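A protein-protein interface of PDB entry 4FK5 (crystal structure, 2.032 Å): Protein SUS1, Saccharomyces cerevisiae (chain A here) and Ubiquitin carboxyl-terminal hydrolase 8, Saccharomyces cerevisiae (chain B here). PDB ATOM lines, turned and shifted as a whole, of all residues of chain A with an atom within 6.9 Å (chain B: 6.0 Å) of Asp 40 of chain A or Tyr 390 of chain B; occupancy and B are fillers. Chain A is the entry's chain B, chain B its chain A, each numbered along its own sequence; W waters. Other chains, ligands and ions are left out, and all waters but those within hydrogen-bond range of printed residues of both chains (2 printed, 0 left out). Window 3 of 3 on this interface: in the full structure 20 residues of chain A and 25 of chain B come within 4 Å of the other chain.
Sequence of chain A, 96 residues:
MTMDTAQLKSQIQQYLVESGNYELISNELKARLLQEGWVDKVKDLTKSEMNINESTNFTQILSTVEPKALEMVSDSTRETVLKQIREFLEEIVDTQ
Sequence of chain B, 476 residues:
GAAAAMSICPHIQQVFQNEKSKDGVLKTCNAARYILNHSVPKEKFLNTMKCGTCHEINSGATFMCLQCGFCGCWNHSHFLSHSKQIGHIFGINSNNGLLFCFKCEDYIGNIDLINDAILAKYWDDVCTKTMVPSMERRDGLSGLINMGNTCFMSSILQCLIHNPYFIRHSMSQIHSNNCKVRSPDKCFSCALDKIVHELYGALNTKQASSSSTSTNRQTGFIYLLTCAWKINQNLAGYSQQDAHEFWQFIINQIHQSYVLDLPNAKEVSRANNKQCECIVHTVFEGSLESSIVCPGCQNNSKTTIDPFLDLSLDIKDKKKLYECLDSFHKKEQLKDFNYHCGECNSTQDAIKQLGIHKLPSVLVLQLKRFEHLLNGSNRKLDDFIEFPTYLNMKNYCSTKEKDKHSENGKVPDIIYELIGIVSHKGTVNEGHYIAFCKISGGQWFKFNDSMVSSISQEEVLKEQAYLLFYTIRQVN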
ATOM      1  N   ALA A  31     -31.659  16.044 -30.895  1.00  0.00           N
ATOM      2  CA  ALA A  31     -32.339  16.420 -29.618  1.00  0.00           C
ATOM      3  C   ALA A  31     -32.720  15.131 -28.845  1.00  0.00           C
ATOM      4  O   ALA A  31     -32.511  15.047 -27.617  1.00  0.00           O
ATOM      5  CB  ALA A  31     -33.596  17.269 -29.873  1.00  0.00           C
ATOM      6  N   LEU A  33     -31.349  12.008 -29.143  1.00  0.00           N
ATOM      7  CA  LEU A  33     -30.158  11.282 -28.721  1.00  0.00           C
ATOM      8  C   LEU A  33     -29.483  11.956 -27.518  1.00  0.00           C
ATOM      9  O   LEU A  33     -28.970  11.299 -26.587  1.00  0.00           O
ATOM     10  CB  LEU A  33     -29.173  11.169 -29.879  1.00  0.00           C
ATOM     11  CG  LEU A  33     -29.598  10.315 -31.059  1.00  0.00           C
ATOM     12  CD1 LEU A  33     -28.521  10.329 -32.197  1.00  0.00           C
ATOM     13  CD2 LEU A  33     -29.876   8.897 -30.564  1.00  0.00           C
ATOM     14  N   LEU A  34     -29.481  13.255 -27.527  1.00  0.00           N
ATOM     15  CA  LEU A  34     -28.907  13.994 -26.451  1.00  0.00           C
ATOM     16  C   LEU A  34     -29.686  13.772 -25.166  1.00  0.00           C
ATOM     17  O   LEU A  34     -29.100  13.460 -24.112  1.00  0.00           O
ATOM     18  CB  LEU A  34     -28.868  15.494 -26.818  1.00  0.00           C
ATOM     19  CG  LEU A  34     -28.301  16.461 -25.836  1.00  0.00           C
ATOM     20  CD1 LEU A  34     -26.806  16.215 -25.721  1.00  0.00           C
ATOM     21  CD2 LEU A  34     -28.600  17.925 -26.289  1.00  0.00           C
ATOM     22  N   GLN A  35     -31.017  13.902 -25.243  1.00  0.00           N
ATOM     23  CA  GLN A  35     -31.875  13.814 -24.061  1.00  0.00           C
ATOM     24  C   GLN A  35     -31.954  12.394 -23.460  1.00  0.00           C
ATOM     25  O   GLN A  35     -32.113  12.232 -22.252  1.00  0.00           O
ATOM     26  CB  GLN A  35     -33.263  14.269 -24.411  1.00  0.00           C
ATOM     27  CG  GLN A  35     -33.435  15.774 -24.302  1.00  0.00           C
ATOM     28  CD  GLN A  35     -34.796  16.225 -24.813  1.00  0.00           C
ATOM     29  OE1 GLN A  35     -35.579  16.702 -24.068  1.00  0.00           O
ATOM     30  NE2 GLN A  35     -35.073  15.991 -26.108  1.00  0.00           N
ATOM     31  N   GLU A  36     -31.844  11.380 -24.285  1.00  0.00           N
ATOM     32  CA  GLU A  36     -31.869  10.007 -23.762  1.00  0.00           C
ATOM     33  C   GLU A  36     -30.485   9.596 -23.210  1.00  0.00           C
ATOM     34  O   GLU A  36     -30.340   8.506 -22.725  1.00  0.00           O
ATOM     35  CB  GLU A  36     -32.380   9.011 -24.825  1.00  0.00           C
ATOM     36  CG  GLU A  36     -31.384   8.633 -25.947  1.00  0.00           C
ATOM     37  CD  GLU A  36     -32.018   7.753 -27.064  1.00  0.00           C
ATOM     38  OE1 GLU A  36     -33.205   7.930 -27.316  1.00  0.00           O
ATOM     39  OE2 GLU A  36     -31.332   6.824 -27.634  1.00  0.00           O
ATOM     40  N   GLY A  37     -29.476  10.460 -23.369  1.00  0.00           N
ATOM     41  CA  GLY A  37     -28.129  10.206 -22.837  1.00  0.00           C
ATOM     42  C   GLY A  37     -27.147   9.458 -23.750  1.00  0.00           C
ATOM     43  O   GLY A  37     -26.020   9.085 -23.314  1.00  0.00           O
ATOM     44  N   TRP A  38     -27.548   9.230 -24.999  1.00  0.00           N
ATOM     45  CA  TRP A  38     -26.764   8.478 -25.938  1.00  0.00           C
ATOM     46  C   TRP A  38     -25.485   9.195 -26.335  1.00  0.00           C
ATOM     47  O   TRP A  38     -24.431   8.560 -26.493  1.00  0.00           O
ATOM     48  CB  TRP A  38     -27.604   8.181 -27.168  1.00  0.00           C
ATOM     49  CG  TRP A  38     -26.865   7.508 -28.291  1.00  0.00           C
ATOM     50  CD1 TRP A  38     -26.852   6.162 -28.591  1.00  0.00           C
ATOM     51  CD2 TRP A  38     -26.083   8.141 -29.356  1.00  0.00           C
ATOM     52  NE1 TRP A  38     -26.186   5.938 -29.781  1.00  0.00           N
ATOM     53  CE2 TRP A  38     -25.692   7.081 -30.268  1.00  0.00           C
ATOM     54  CE3 TRP A  38     -25.727   9.440 -29.653  1.00  0.00           C
ATOM     55  CZ2 TRP A  38     -24.942   7.321 -31.393  1.00  0.00           C
ATOM     56  CZ3 TRP A  38     -24.997   9.687 -30.823  1.00  0.00           C
ATOM     57  CH2 TRP A  38     -24.611   8.654 -31.663  1.00  0.00           C
ATOM     58  N   VAL A  39     -25.537  10.510 -26.461  1.00  0.00           N
ATOM     59  CA  VAL A  39     -24.324  11.300 -26.804  1.00  0.00           C
ATOM     60  C   VAL A  39     -23.205  11.046 -25.735  1.00  0.00           C
ATOM     61  O   VAL A  39     -22.048  10.722 -26.061  1.00  0.00           O
ATOM     62  CB  VAL A  39     -24.628  12.793 -26.952  1.00  0.00           C
ATOM     63  CG1 VAL A  39     -23.324  13.619 -27.084  1.00  0.00           C
ATOM     64  CG2 VAL A  39     -25.508  13.032 -28.190  1.00  0.00           C
ATOM     65  N   ASP A  40     -23.580  11.115 -24.492  1.00  0.00           N
ATOM     66  CA  ASP A  40     -22.604  10.955 -23.428  1.00  0.00           C
ATOM     67  C   ASP A  40     -22.162   9.504 -23.231  1.00  0.00           C
ATOM     68  O   ASP A  40     -21.028   9.245 -22.866  1.00  0.00           O
ATOM     69  CB  ASP A  40     -23.157  11.584 -22.161  1.00  0.00           C
ATOM     70  CG  ASP A  40     -23.383  13.047 -22.348  1.00  0.00           C
ATOM     71  OD1 ASP A  40     -22.486  13.698 -22.977  1.00  0.00           O
ATOM     72  OD2 ASP A  40     -24.470  13.529 -22.079  1.00  0.00           O
ATOM     73  N   LYS A  41     -23.051   8.579 -23.546  1.00  0.00           N
ATOM     74  CA  LYS A  41     -22.716   7.166 -23.586  1.00  0.00           C
ATOM     75  C   LYS A  41     -21.689   6.884 -24.660  1.00  0.00           C
ATOM     76  O   LYS A  41     -20.803   6.064 -24.454  1.00  0.00           O
ATOM     77  CB  LYS A  41     -23.948   6.319 -23.889  1.00  0.00           C
ATOM     78  CG  LYS A  41     -24.483   5.539 -22.732  1.00  0.00           C
ATOM     79  CD  LYS A  41     -25.441   6.362 -21.899  1.00  0.00           C
ATOM     80  CE  LYS A  41     -26.404   5.485 -21.087  1.00  0.00           C
ATOM     81  NZ  LYS A  41     -25.686   4.680 -20.035  1.00  0.00           N
ATOM     82  N   VAL A  42     -21.809   7.539 -25.825  1.00  0.00           N
ATOM     83  CA  VAL A  42     -20.859   7.291 -26.909  1.00  0.00           C
ATOM     84  C   VAL A  42     -19.480   7.874 -26.559  1.00  0.00           C
ATOM     85  O   VAL A  42     -18.443   7.252 -26.834  1.00  0.00           O
ATOM     86  CB  VAL A  42     -21.357   7.816 -28.257  1.00  0.00           C
ATOM     87  CG1 VAL A  42     -20.265   7.729 -29.317  1.00  0.00           C
ATOM     88  CG2 VAL A  42     -22.603   7.059 -28.659  1.00  0.00           C
ATOM     89  N   LYS A  43     -19.477   8.997 -25.882  1.00  0.00           N
ATOM     90  CA  LYS A  43     -18.253   9.585 -25.422  1.00  0.00           C
ATOM     91  C   LYS A  43     -17.552   8.661 -24.359  1.00  0.00           C
ATOM     92  O   LYS A  43     -16.367   8.439 -24.439  1.00  0.00           O
ATOM     93  CB  LYS A  43     -18.507  10.952 -24.823  1.00  0.00           C
ATOM     94  CG  LYS A  43     -18.858  11.988 -25.874  1.00  0.00           C
ATOM     95  CD  LYS A  43     -19.093  13.354 -25.288  1.00  0.00           C
ATOM     96  CE  LYS A  43     -19.660  14.299 -26.374  1.00  0.00           C
ATOM     97  NZ  LYS A  43     -19.609  15.705 -25.956  1.00  0.00           N
ATOM     98  N   ASP A  44     -18.311   8.158 -23.398  1.00  0.00           N
ATOM     99  CA  ASP A  44     -17.780   7.138 -22.450  1.00  0.00           C
ATOM    100  C   ASP A  44     -17.208   5.914 -23.149  1.00  0.00           C
ATOM    101  O   ASP A  44     -16.082   5.503 -22.857  1.00  0.00           O
ATOM    102  CB  ASP A  44     -18.835   6.709 -21.483  1.00  0.00           C
ATOM    103  CG  ASP A  44     -19.219   7.813 -20.525  1.00  0.00           C
ATOM    104  OD1 ASP A  44     -18.356   8.723 -20.286  1.00  0.00           O
ATOM    105  OD2 ASP A  44     -20.381   7.779 -20.002  1.00  0.00           O
ATOM    106  N   LEU A  45     -17.988   5.329 -24.048  1.00  0.00           N
ATOM    107  CA  LEU A  45     -17.579   4.165 -24.773  1.00  0.00           C
ATOM    108  C   LEU A  45     -16.262   4.459 -25.480  1.00  0.00           C
ATOM    109  O   LEU A  45     -15.373   3.639 -25.502  1.00  0.00           O
ATOM    110  CB  LEU A  45     -18.677   3.733 -25.762  1.00  0.00           C
ATOM    111  CG  LEU A  45     -18.348   2.691 -26.852  1.00  0.00           C
ATOM    112  CD1 LEU A  45     -17.831   1.386 -26.216  1.00  0.00           C
ATOM    113  CD2 LEU A  45     -19.585   2.434 -27.758  1.00  0.00           C
ATOM    114  N   THR A  46     -16.115   5.664 -25.984  1.00  0.00           N
ATOM    115  CA  THR A  46     -14.944   6.006 -26.758  1.00  0.00           C
ATOM    116  C   THR A  46     -13.717   6.066 -25.852  1.00  0.00           C
ATOM    117  O   THR A  46     -12.695   5.477 -26.180  1.00  0.00           O
ATOM    118  CB  THR A  46     -15.130   7.309 -27.538  1.00  0.00           C
ATOM    119  OG1 THR A  46     -16.253   7.155 -28.440  1.00  0.00           O
ATOM    120  CG2 THR A  46     -13.894   7.613 -28.345  1.00  0.00           C
ATOM    121  N   MET A  72     -26.678   1.118 -29.621  1.00  0.00           N
ATOM    122  CA  MET A  72     -27.103   1.753 -28.378  1.00  0.00           C
ATOM    123  C   MET A  72     -28.267   2.732 -28.590  1.00  0.00           C
ATOM    124  O   MET A  72     -28.829   3.197 -27.634  1.00  0.00           O
ATOM    125  CB  MET A  72     -25.963   2.502 -27.731  1.00  0.00           C
ATOM    126  CG  MET A  72     -24.879   1.630 -27.101  1.00  0.00           C
ATOM    127  SD  MET A  72     -23.414   2.628 -26.788  1.00  0.00           S
ATOM    128  CE  MET A  72     -23.906   3.489 -25.321  1.00  0.00           C
ATOM    129  N   TYR B 322     -39.797  18.839 -13.387  1.00  0.00           N
ATOM    130  CA  TYR B 322     -40.753  19.246 -14.426  1.00  0.00           C
ATOM    131  C   TYR B 322     -42.157  19.531 -13.770  1.00  0.00           C
ATOM    132  O   TYR B 322     -42.844  20.503 -14.148  1.00  0.00           O
ATOM    133  CB  TYR B 322     -40.898  18.153 -15.525  1.00  0.00           C
ATOM    134  CG  TYR B 322     -39.827  18.171 -16.593  1.00  0.00           C
ATOM    135  CD1 TYR B 322     -39.617  19.308 -17.386  1.00  0.00           C
ATOM    136  CD2 TYR B 322     -39.030  17.061 -16.821  1.00  0.00           C
ATOM    137  CE1 TYR B 322     -38.681  19.307 -18.389  1.00  0.00           C
ATOM    138  CE2 TYR B 322     -38.060  17.064 -17.814  1.00  0.00           C
ATOM    139  CZ  TYR B 322     -37.897  18.188 -18.605  1.00  0.00           C
ATOM    140  OH  TYR B 322     -36.942  18.191 -19.597  1.00  0.00           O
ATOM    141  N   PRO B 388     -33.162  16.417 -14.228  1.00  0.00           N
ATOM    142  CA  PRO B 388     -32.605  15.678 -15.359  1.00  0.00           C
ATOM    143  C   PRO B 388     -31.235  16.213 -15.749  1.00  0.00           C
ATOM    144  O   PRO B 388     -30.916  17.399 -15.484  1.00  0.00           O
ATOM    145  CB  PRO B 388     -33.635  15.922 -16.457  1.00  0.00           C
ATOM    146  CG  PRO B 388     -34.140  17.299 -16.161  1.00  0.00           C
ATOM    147  CD  PRO B 388     -34.208  17.359 -14.659  1.00  0.00           C
ATOM    148  N   THR B 389     -30.433  15.366 -16.358  1.00  0.00           N
ATOM    149  CA  THR B 389     -29.111  15.783 -16.908  1.00  0.00           C
ATOM    150  C   THR B 389     -29.297  16.764 -18.102  1.00  0.00           C
ATOM    151  O   THR B 389     -28.450  17.605 -18.335  1.00  0.00           O
ATOM    152  CB  THR B 389     -28.277  14.582 -17.402  1.00  0.00           C
ATOM    153  OG1 THR B 389     -29.062  13.819 -18.330  1.00  0.00           O
ATOM    154  CG2 THR B 389     -27.846  13.666 -16.243  1.00  0.00           C
ATOM    155  N   TYR B 390     -30.391  16.611 -18.855  1.00  0.00           N
ATOM    156  CA  TYR B 390     -30.760  17.557 -19.899  1.00  0.00           C
ATOM    157  C   TYR B 390     -32.219  18.034 -19.687  1.00  0.00           C
ATOM    158  O   TYR B 390     -33.124  17.247 -19.426  1.00  0.00           O
ATOM    159  CB  TYR B 390     -30.565  16.904 -21.302  1.00  0.00           C
ATOM    160  CG  TYR B 390     -29.144  16.668 -21.588  1.00  0.00           C
ATOM    161  CD1 TYR B 390     -28.347  17.677 -22.066  1.00  0.00           C
ATOM    162  CD2 TYR B 390     -28.524  15.436 -21.267  1.00  0.00           C
ATOM    163  CE1 TYR B 390     -26.999  17.479 -22.289  1.00  0.00           C
ATOM    164  CE2 TYR B 390     -27.147  15.251 -21.486  1.00  0.00           C
ATOM    165  CZ  TYR B 390     -26.403  16.270 -21.998  1.00  0.00           C
ATOM    166  OH  TYR B 390     -25.045  16.106 -22.223  1.00  0.00           O
ATOM    167  N   LEU B 391     -32.420  19.310 -19.748  1.00  0.00           N
ATOM    168  CA  LEU B 391     -33.700  19.911 -19.400  1.00  0.00           C
ATOM    169  C   LEU B 391     -34.265  20.607 -20.596  1.00  0.00           C
ATOM    170  O   LEU B 391     -33.603  21.507 -21.143  1.00  0.00           O
ATOM    171  CB  LEU B 391     -33.462  20.929 -18.387  1.00  0.00           C
ATOM    172  CG  LEU B 391     -34.510  21.513 -17.439  1.00  0.00           C
ATOM    173  CD1 LEU B 391     -34.343  22.969 -17.257  1.00  0.00           C
ATOM    174  CD2 LEU B 391     -35.946  20.978 -17.373  1.00  0.00           C
ATOM    175  N   ASN B 392     -35.523  20.307 -20.928  1.00  0.00           N
ATOM    176  CA  ASN B 392     -36.195  20.897 -22.119  1.00  0.00           C
ATOM    177  C   ASN B 392     -37.173  21.917 -21.616  1.00  0.00           C
ATOM    178  O   ASN B 392     -38.104  21.560 -20.901  1.00  0.00           O
ATOM    179  CB  ASN B 392     -36.941  19.834 -22.908  1.00  0.00           C
ATOM    180  CG  ASN B 392     -37.335  20.305 -24.294  1.00  0.00           C
ATOM    181  OD1 ASN B 392     -37.496  21.505 -24.528  1.00  0.00           O
ATOM    182  ND2 ASN B 392     -37.415  19.343 -25.268  1.00  0.00           N
ATOM    183  N   ILE B 415     -33.061  22.890 -25.182  1.00  0.00           N
ATOM    184  CA  ILE B 415     -32.495  21.905 -24.259  1.00  0.00           C
ATOM    185  C   ILE B 415     -31.214  22.410 -23.597  1.00  0.00           C
ATOM    186  O   ILE B 415     -30.220  22.824 -24.305  1.00  0.00           O
ATOM    187  CB  ILE B 415     -32.179  20.627 -24.971  1.00  0.00           C
ATOM    188  CG1 ILE B 415     -33.471  19.946 -25.508  1.00  0.00           C
ATOM    189  CG2 ILE B 415     -31.426  19.663 -24.041  1.00  0.00           C
ATOM    190  CD1 ILE B 415     -33.183  18.943 -26.611  1.00  0.00           C
ATOM    191  N   TYR B 416     -31.214  22.379 -22.262  1.00  0.00           N
ATOM    192  CA  TYR B 416     -30.097  22.823 -21.447  1.00  0.00           C
ATOM    193  C   TYR B 416     -29.373  21.599 -20.881  1.00  0.00           C
ATOM    194  O   TYR B 416     -30.011  20.555 -20.607  1.00  0.00           O
ATOM    195  CB  TYR B 416     -30.624  23.655 -20.252  1.00  0.00           C
ATOM    196  CG  TYR B 416     -31.104  25.052 -20.566  1.00  0.00           C
ATOM    197  CD1 TYR B 416     -32.371  25.280 -21.048  1.00  0.00           C
ATOM    198  CD2 TYR B 416     -30.274  26.152 -20.321  1.00  0.00           C
ATOM    199  CE1 TYR B 416     -32.814  26.559 -21.321  1.00  0.00           C
ATOM    200  CE2 TYR B 416     -30.685  27.426 -20.581  1.00  0.00           C
ATOM    201  CZ  TYR B 416     -31.973  27.630 -21.080  1.00  0.00           C
ATOM    202  OH  TYR B 416     -32.352  28.896 -21.328  1.00  0.00           O
ATOM    203  N   GLU B 417     -28.075  21.747 -20.640  1.00  0.00           N
ATOM    204  CA  GLU B 417     -27.265  20.720 -20.008  1.00  0.00           C
ATOM    205  C   GLU B 417     -27.013  21.116 -18.572  1.00  0.00           C
ATOM    206  O   GLU B 417     -26.505  22.211 -18.297  1.00  0.00           O
ATOM    207  CB  GLU B 417     -25.945  20.539 -20.801  1.00  0.00           C
ATOM    208  CG  GLU B 417     -24.855  19.667 -20.161  1.00  0.00           C
ATOM    209  CD  GLU B 417     -23.622  19.499 -21.074  1.00  0.00           C
ATOM    210  OE1 GLU B 417     -22.759  18.652 -20.738  1.00  0.00           O
ATOM    211  OE2 GLU B 417     -23.493  20.251 -22.113  1.00  0.00           O
ATOM    212  N   LEU B 418     -27.317  20.220 -17.650  1.00  0.00           N
ATOM    213  CA  LEU B 418     -26.921  20.393 -16.213  1.00  0.00           C
ATOM    214  C   LEU B 418     -25.410  20.406 -15.998  1.00  0.00           C
ATOM    215  O   LEU B 418     -24.706  19.462 -16.408  1.00  0.00           O
ATOM    216  CB  LEU B 418     -27.533  19.268 -15.353  1.00  0.00           C
ATOM    217  CG  LEU B 418     -27.250  19.402 -13.845  1.00  0.00           C
ATOM    218  CD1 LEU B 418     -27.958  20.619 -13.241  1.00  0.00           C
ATOM    219  CD2 LEU B 418     -27.620  18.094 -13.165  1.00  0.00           C
ATOM    220  N   LYS B 438     -19.861  19.631 -13.205  1.00  0.00           N
ATOM    221  CA  LYS B 438     -19.553  18.766 -14.336  1.00  0.00           C
ATOM    222  C   LYS B 438     -18.548  19.519 -15.183  1.00  0.00           C
ATOM    223  O   LYS B 438     -18.720  20.701 -15.454  1.00  0.00           O
ATOM    224  CB  LYS B 438     -20.816  18.506 -15.174  1.00  0.00           C
ATOM    225  CG  LYS B 438     -20.703  17.356 -16.165  1.00  0.00           C
ATOM    226  CD  LYS B 438     -22.045  17.177 -16.942  1.00  0.00           C
ATOM    227  CE  LYS B 438     -21.830  16.994 -18.397  1.00  0.00           C
ATOM    228  NZ  LYS B 438     -23.087  16.633 -19.145  1.00  0.00           N
ATOM    229  N   GLN B 457     -22.083  10.155 -12.100  1.00  0.00           N
ATOM    230  CA  GLN B 457     -23.335  10.784 -12.400  1.00  0.00           C
ATOM    231  C   GLN B 457     -24.536  10.175 -11.629  1.00  0.00           C
ATOM    232  O   GLN B 457     -25.376  10.936 -11.080  1.00  0.00           O
ATOM    233  CB  GLN B 457     -23.568  10.726 -13.865  1.00  0.00           C
ATOM    234  CG  GLN B 457     -24.819  11.423 -14.321  1.00  0.00           C
ATOM    235  CD  GLN B 457     -24.769  11.697 -15.781  1.00  0.00           C
ATOM    236  OE1 GLN B 457     -24.091  12.632 -16.237  1.00  0.00           O
ATOM    237  NE2 GLN B 457     -25.448  10.886 -16.537  1.00  0.00           N
ATOM    238  N   TYR B 470     -27.849  25.256 -15.254  1.00  0.00           N
ATOM    239  CA  TYR B 470     -28.124  24.638 -16.573  1.00  0.00           C
ATOM    240  C   TYR B 470     -27.592  25.591 -17.662  1.00  0.00           C
ATOM    241  O   TYR B 470     -27.874  26.797 -17.631  1.00  0.00           O
ATOM    242  CB  TYR B 470     -29.613  24.455 -16.768  1.00  0.00           C
ATOM    243  CG  TYR B 470     -30.196  23.197 -16.136  1.00  0.00           C
ATOM    244  CD1 TYR B 470     -30.076  21.958 -16.768  1.00  0.00           C
ATOM    245  CD2 TYR B 470     -30.809  23.232 -14.884  1.00  0.00           C
ATOM    246  CE1 TYR B 470     -30.592  20.824 -16.212  1.00  0.00           C
ATOM    247  CE2 TYR B 470     -31.364  22.070 -14.318  1.00  0.00           C
ATOM    248  CZ  TYR B 470     -31.237  20.884 -14.977  1.00  0.00           C
ATOM    249  OH  TYR B 470     -31.717  19.761 -14.405  1.00  0.00           O
ATOM    250  N   ARG B 473     -27.694  24.213 -24.573  1.00  0.00           N
ATOM    251  CA  ARG B 473     -26.930  23.179 -25.337  1.00  0.00           C
ATOM    252  C   ARG B 473     -27.488  22.992 -26.750  1.00  0.00           C
ATOM    253  O   ARG B 473     -26.708  22.920 -27.719  1.00  0.00           O
ATOM    254  CB  ARG B 473     -26.878  21.861 -24.545  1.00  0.00           C
ATOM    255  CG  ARG B 473     -26.162  20.683 -25.231  1.00  0.00           C
ATOM    256  CD  ARG B 473     -24.686  20.954 -25.425  1.00  0.00           C
ATOM    257  NE  ARG B 473     -24.094  19.831 -26.086  1.00  0.00           N
ATOM    258  CZ  ARG B 473     -23.893  18.665 -25.498  1.00  0.00           C
ATOM    259  NH1 ARG B 473     -24.030  18.546 -24.175  1.00  0.00           N
ATOM    260  NH2 ARG B 473     -23.442  17.639 -26.193  1.00  0.00           N
HETATM  261  O   HOH W   1     -22.209  15.753 -24.230  1.00  0.00           O
HETATM  262  O   HOH W   2     -21.932  14.301 -19.693  1.00  0.00           O
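Of chain B, only Tyr 390 (2.6 Å) comes within 4 Å of Asp 40 of chain A.
Of the printed residues of chain A, Tyr 390 of chain B touches Leu 34 and Asp 40.
Of the printed residues of chain A, Ile 415 of chain B touches Ala 31 and Gln 35.
Of the printed residues of chain A, Arg 473 of chain B touches Leu 34 (3.7 Å).
Of the printed residues of chain B, Gln 35 of chain A touches Asn 392 (3.4 Å) and Ile 415 (3.5 Å).
The nearest printed residue of chain B that does not touch Leu 34 of chain A is Ile 415 of chain B (4.01 Å).
Ala 31 of chain A touches Ile 415 of chain B (CB to CD1, 3.7 Å).
Tyr 390 of chain B touches Leu 34 of chain A.
Leu 34 of chain A touches Arg 473 of chain B (CD1 to NH2, 3.7 Å).
CD1 of Ile 415 of chain B touches NE2 of Gln 35 of chain A, 3.5 Å away.
OH of Tyr 390 of chain B is in hydrogen-bond range of NH1 of Arg 473 of chain B (3.3 Å).
The backbone carbonyl oxygen (O) of Ala 31 of chain A lies within hydrogen-bond range of the side-chain amide nitrogen (NE2) of Gln 35 of chain A.
NH1 of Arg 473 of chain B is in salt-bridge range of OE2 of Glu 417 of chain B, 2.7 Å away.
The side-chain hydroxyl (OH) of Tyr 322 of chain B lies within hydrogen-bond range of the backbone NH (N) of Asn 392 of chain B.
The backbone NH of Arg 473 of chain B sits at hydrogen-bond distance from the backbone carbonyl oxygen of Ile 415 of chain B.
The side-chain amide nitrogen (ND2) of Asn 392 of chain B lies within hydrogen-bond range of the side-chain amide oxygen (OE1) of Gln 35 of chain A (3.4 Å).
The side-chain hydroxyl of Tyr 390 of chain B lies within hydrogen-bond range of the side-chain carboxylate of Asp 40 of chain A (2.6 Å).
Water W1 lies within hydrogen-bond range of the side-chain carboxylate of Asp 40 of chain A (2.4 Å), the guanidinium group of Arg 473 of chain B (3.0 Å), the side-chain amino group of Lys 43 of chain A (3.1 Å) and the side-chain hydroxyl of Tyr 390 of chain B (3.5 Å).
Water W2 lies within hydrogen-bond range of the side-chain amino group of Lys 438 of chain B (2.7 Å) and the side-chain carboxylate of Asp 40 of chain A (3.4 Å).
Hydrophobic or aromatic side chains of chain B within 4 Å of the printed part of chain A: Tyr 390 and Ile 415.
Of the 16 printed residues of chain A, 4 touch a printed residue of chain B.
Among the printed residues, 6 pairs touch across the chains.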
